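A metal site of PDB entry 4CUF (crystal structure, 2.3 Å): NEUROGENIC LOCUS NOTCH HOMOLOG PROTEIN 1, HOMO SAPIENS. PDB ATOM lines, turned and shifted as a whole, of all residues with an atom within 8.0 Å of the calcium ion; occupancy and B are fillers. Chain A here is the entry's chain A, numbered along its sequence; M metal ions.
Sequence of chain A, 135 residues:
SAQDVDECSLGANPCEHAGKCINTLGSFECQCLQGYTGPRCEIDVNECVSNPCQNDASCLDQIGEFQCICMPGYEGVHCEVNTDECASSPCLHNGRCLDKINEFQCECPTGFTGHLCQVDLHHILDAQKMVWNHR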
ATOM      1  N   PRO A  72      -0.538 -22.428 -26.795  1.00  0.00           N
ATOM      2  CA  PRO A  72      -1.694 -21.507 -26.639  1.00  0.00           C
ATOM      3  C   PRO A  72      -2.830 -22.153 -25.864  1.00  0.00           C
ATOM      4  O   PRO A  72      -3.138 -23.332 -26.098  1.00  0.00           O
ATOM      5  CB  PRO A  72      -2.126 -21.232 -28.082  1.00  0.00           C
ATOM      6  CG  PRO A  72      -0.920 -21.538 -28.908  1.00  0.00           C
ATOM      7  CD  PRO A  72      -0.163 -22.613 -28.215  1.00  0.00           C
ATOM      8  N   GLY A  73      -3.398 -21.419 -24.925  1.00  0.00           N
ATOM      9  CA  GLY A  73      -4.489 -21.932 -24.106  1.00  0.00           C
ATOM     10  C   GLY A  73      -4.078 -22.462 -22.754  1.00  0.00           C
ATOM     11  O   GLY A  73      -4.921 -22.782 -21.916  1.00  0.00           O
ATOM     12  N   TYR A  74      -2.769 -22.556 -22.526  1.00  0.00           N
ATOM     13  CA  TYR A  74      -2.216 -23.033 -21.256  1.00  0.00           C
ATOM     14  C   TYR A  74      -1.448 -21.943 -20.558  1.00  0.00           C
ATOM     15  O   TYR A  74      -0.942 -21.035 -21.198  1.00  0.00           O
ATOM     16  CB  TYR A  74      -1.357 -24.283 -21.445  1.00  0.00           C
ATOM     17  CG  TYR A  74      -2.133 -25.450 -21.972  1.00  0.00           C
ATOM     18  CD1 TYR A  74      -2.839 -26.291 -21.117  1.00  0.00           C
ATOM     19  CD2 TYR A  74      -2.219 -25.699 -23.347  1.00  0.00           C
ATOM     20  CE1 TYR A  74      -3.590 -27.347 -21.604  1.00  0.00           C
ATOM     21  CE2 TYR A  74      -2.966 -26.762 -23.842  1.00  0.00           C
ATOM     22  CZ  TYR A  74      -3.646 -27.589 -22.971  1.00  0.00           C
ATOM     23  OH  TYR A  74      -4.339 -28.670 -23.464  1.00  0.00           O
ATOM     24  N   VAL A  81      -2.163 -25.326 -16.207  1.00  0.00           N
ATOM     25  CA  VAL A  81      -3.488 -24.713 -16.184  1.00  0.00           C
ATOM     26  C   VAL A  81      -4.016 -24.480 -17.593  1.00  0.00           C
ATOM     27  O   VAL A  81      -3.400 -23.767 -18.403  1.00  0.00           O
ATOM     28  CB  VAL A  81      -3.456 -23.389 -15.407  1.00  0.00           C
ATOM     29  CG1 VAL A  81      -4.803 -22.663 -15.471  1.00  0.00           C
ATOM     30  CG2 VAL A  81      -2.987 -23.595 -13.993  1.00  0.00           C
ATOM     31  N   ASN A  82      -5.185 -25.052 -17.855  1.00  0.00           N
ATOM     32  CA  ASN A  82      -5.935 -24.851 -19.069  1.00  0.00           C
ATOM     33  C   ASN A  82      -6.757 -23.600 -18.775  1.00  0.00           C
ATOM     34  O   ASN A  82      -7.658 -23.637 -17.955  1.00  0.00           O
ATOM     35  CB  ASN A  82      -6.790 -26.078 -19.332  1.00  0.00           C
ATOM     36  CG  ASN A  82      -7.607 -25.989 -20.592  1.00  0.00           C
ATOM     37  OD1 ASN A  82      -8.121 -24.924 -20.947  1.00  0.00           O
ATOM     38  ND2 ASN A  82      -7.803 -27.117 -21.242  1.00  0.00           N
ATOM     39  N   THR A  83      -6.394 -22.466 -19.377  1.00  0.00           N
ATOM     40  CA  THR A  83      -7.079 -21.182 -19.176  1.00  0.00           C
ATOM     41  C   THR A  83      -8.583 -21.318 -19.374  1.00  0.00           C
ATOM     42  O   THR A  83      -9.017 -21.947 -20.351  1.00  0.00           O
ATOM     43  CB  THR A  83      -6.517 -20.143 -20.189  1.00  0.00           C
ATOM     44  OG1 THR A  83      -5.078 -20.014 -20.017  1.00  0.00           O
ATOM     45  CG2 THR A  83      -7.238 -18.780 -20.094  1.00  0.00           C
ATOM     46  N   ASP A  84      -9.384 -20.762 -18.461  1.00  0.00           N
ATOM     47  CA  ASP A  84     -10.834 -20.843 -18.610  1.00  0.00           C
ATOM     48  C   ASP A  84     -11.408 -19.744 -19.510  1.00  0.00           C
ATOM     49  O   ASP A  84     -11.675 -18.634 -19.050  1.00  0.00           O
ATOM     50  CB  ASP A  84     -11.526 -20.872 -17.253  1.00  0.00           C
ATOM     51  CG  ASP A  84     -13.050 -21.084 -17.301  1.00  0.00           C
ATOM     52  OD1 ASP A  84     -13.578 -21.467 -18.381  1.00  0.00           O
ATOM     53  OD2 ASP A  84     -13.694 -20.922 -16.259  1.00  0.00           O
ATOM     54  N   GLU A  85     -11.691 -20.061 -20.762  1.00  0.00           N
ATOM     55  CA  GLU A  85     -12.267 -19.080 -21.699  1.00  0.00           C
ATOM     56  C   GLU A  85     -13.759 -18.733 -21.436  1.00  0.00           C
ATOM     57  O   GLU A  85     -14.294 -17.754 -21.970  1.00  0.00           O
ATOM     58  CB  GLU A  85     -12.024 -19.486 -23.169  1.00  0.00           C
ATOM     59  CG  GLU A  85     -10.565 -19.301 -23.610  1.00  0.00           C
ATOM     60  CD  GLU A  85      -9.602 -20.443 -23.320  1.00  0.00           C
ATOM     61  OE1 GLU A  85     -10.089 -21.588 -23.180  1.00  0.00           O
ATOM     62  OE2 GLU A  85      -8.370 -20.203 -23.226  1.00  0.00           O
ATOM     63  N   CYS A  86     -14.397 -19.522 -20.581  1.00  0.00           N
ATOM     64  CA  CYS A  86     -15.793 -19.322 -20.221  1.00  0.00           C
ATOM     65  C   CYS A  86     -15.938 -18.384 -19.054  1.00  0.00           C
ATOM     66  O   CYS A  86     -17.055 -17.992 -18.732  1.00  0.00           O
ATOM     67  CB  CYS A  86     -16.470 -20.662 -19.950  1.00  0.00           C
ATOM     68  SG  CYS A  86     -16.711 -21.668 -21.440  1.00  0.00           S
ATOM     69  N   LEU A  98     -18.881 -24.181 -23.066  1.00  0.00           N
ATOM     70  CA  LEU A  98     -17.946 -25.295 -22.963  1.00  0.00           C
ATOM     71  C   LEU A  98     -16.539 -24.788 -23.192  1.00  0.00           C
ATOM     72  O   LEU A  98     -16.269 -24.177 -24.228  1.00  0.00           O
ATOM     73  CB  LEU A  98     -18.268 -26.405 -23.986  1.00  0.00           C
ATOM     74  CG  LEU A  98     -17.366 -27.682 -23.996  1.00  0.00           C
ATOM     75  CD1 LEU A  98     -17.204 -28.304 -22.597  1.00  0.00           C
ATOM     76  CD2 LEU A  98     -17.980 -28.727 -24.907  1.00  0.00           C
ATOM     77  N   ASP A  99     -15.632 -25.021 -22.219  1.00  0.00           N
ATOM     78  CA  ASP A  99     -14.273 -24.562 -22.309  1.00  0.00           C
ATOM     79  C   ASP A  99     -13.484 -25.535 -23.175  1.00  0.00           C
ATOM     80  O   ASP A  99     -13.624 -26.763 -23.057  1.00  0.00           O
ATOM     81  CB  ASP A  99     -13.604 -24.450 -20.890  1.00  0.00           C
ATOM     82  CG  ASP A  99     -12.178 -23.933 -20.956  1.00  0.00           C
ATOM     83  OD1 ASP A  99     -11.979 -22.796 -21.411  1.00  0.00           O
ATOM     84  OD2 ASP A  99     -11.264 -24.691 -20.614  1.00  0.00           O
ATOM     85  N   LYS A 100     -12.689 -24.956 -24.075  1.00  0.00           N
ATOM     86  CA  LYS A 100     -11.847 -25.703 -24.979  1.00  0.00           C
ATOM     87  C   LYS A 100     -10.409 -25.211 -24.827  1.00  0.00           C
ATOM     88  O   LYS A 100     -10.088 -24.515 -23.869  1.00  0.00           O
ATOM     89  CB  LYS A 100     -12.320 -25.536 -26.430  1.00  0.00           C
ATOM     90  CG  LYS A 100     -13.746 -25.911 -26.716  1.00  0.00           C
ATOM     91  CD  LYS A 100     -13.941 -27.404 -26.510  1.00  0.00           C
ATOM     92  CE  LYS A 100     -15.231 -27.878 -27.086  1.00  0.00           C
ATOM     93  NZ  LYS A 100     -14.980 -29.022 -28.020  1.00  0.00           N
ATOM     94  N   ILE A 101      -9.544 -25.593 -25.754  1.00  0.00           N
ATOM     95  CA  ILE A 101      -8.150 -25.184 -25.736  1.00  0.00           C
ATOM     96  C   ILE A 101      -8.028 -23.889 -26.525  1.00  0.00           C
ATOM     97  O   ILE A 101      -8.243 -23.873 -27.733  1.00  0.00           O
ATOM     98  CB  ILE A 101      -7.267 -26.306 -26.282  1.00  0.00           C
ATOM     99  CG1 ILE A 101      -7.531 -27.601 -25.478  1.00  0.00           C
ATOM    100  CG2 ILE A 101      -5.765 -25.879 -26.168  1.00  0.00           C
ATOM    101  CD1 ILE A 101      -7.112 -28.910 -26.127  1.00  0.00           C
ATOM    102  N   ASN A 102      -7.775 -22.772 -25.808  1.00  0.00           N
ATOM    103  CA  ASN A 102      -7.661 -21.412 -26.339  1.00  0.00           C
ATOM    104  C   ASN A 102      -8.937 -21.005 -27.093  1.00  0.00           C
ATOM    105  O   ASN A 102      -8.881 -20.279 -28.083  1.00  0.00           O
ATOM    106  CB  ASN A 102      -6.398 -21.319 -27.232  1.00  0.00           C
ATOM    107  CG  ASN A 102      -5.924 -19.924 -27.498  1.00  0.00           C
ATOM    108  OD1 ASN A 102      -6.133 -18.995 -26.691  1.00  0.00           O
ATOM    109  ND2 ASN A 102      -5.242 -19.743 -28.638  1.00  0.00           N
ATOM    110  N   GLU A 103     -10.088 -21.525 -26.663  1.00  0.00           N
ATOM    111  CA  GLU A 103     -11.377 -21.346 -27.326  1.00  0.00           C
ATOM    112  C   GLU A 103     -12.507 -21.742 -26.388  1.00  0.00           C
ATOM    113  O   GLU A 103     -12.271 -22.348 -25.332  1.00  0.00           O
ATOM    114  CB  GLU A 103     -11.447 -22.325 -28.535  1.00  0.00           C
ATOM    115  CG  GLU A 103     -11.259 -21.788 -29.939  1.00  0.00           C
ATOM    116  CD  GLU A 103     -10.535 -22.804 -30.810  1.00  0.00           C
ATOM    117  OE1 GLU A 103     -10.800 -24.014 -30.643  1.00  0.00           O
ATOM    118  OE2 GLU A 103      -9.720 -22.392 -31.661  1.00  0.00           O
ATOM    119  N   PHE A 104     -13.751 -21.438 -26.808  1.00  0.00           N
ATOM    120  CA  PHE A 104     -14.950 -21.868 -26.107  1.00  0.00           C
ATOM    121  C   PHE A 104     -16.000 -22.210 -27.154  1.00  0.00           C
ATOM    122  O   PHE A 104     -15.942 -21.728 -28.280  1.00  0.00           O
ATOM    123  CB  PHE A 104     -15.469 -20.819 -25.088  1.00  0.00           C
ATOM    124  CG  PHE A 104     -15.928 -19.530 -25.728  1.00  0.00           C
ATOM    125  CD1 PHE A 104     -17.216 -19.411 -26.261  1.00  0.00           C
ATOM    126  CD2 PHE A 104     -15.055 -18.456 -25.854  1.00  0.00           C
ATOM    127  CE1 PHE A 104     -17.617 -18.235 -26.882  1.00  0.00           C
ATOM    128  CE2 PHE A 104     -15.465 -17.289 -26.457  1.00  0.00           C
ATOM    129  CZ  PHE A 104     -16.745 -17.179 -26.962  1.00  0.00           C
HETATM  130 CA    CA M   1      -9.583 -23.534 -21.929  1.00  0.00          CA
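OE1 of Glu 85 lies close to N of Glu 103. The backbone NH of Thr 83 lies within hydrogen-bond range of the backbone carbonyl oxygen of Gly 73 (3.0 Å). N of Asp 99 sits at hydrogen-bond distance from SG of Cys 86 (3.6 Å).
Five residues have an atom within 4 Å of the calcium ion: Asn 82, Thr 83, Glu 85, Asp 99 and Lys 100.
The calcium ion is bound by the backbone carbonyl oxygen (O) of Lys 100 (2.2 Å), the side-chain amide oxygen (OD1) of Asn 82 (2.2 Å), the backbone carbonyl oxygen (O) of Thr 83 (2.3 Å), the side-chain carboxylate (OE1) of Glu 85 (2.4 Å), the side-chain carboxylate (OD2) of Asp 99 (2.4 Å) and the side-chain carboxylate (OD1) of Asp 99 (2.6 Å).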
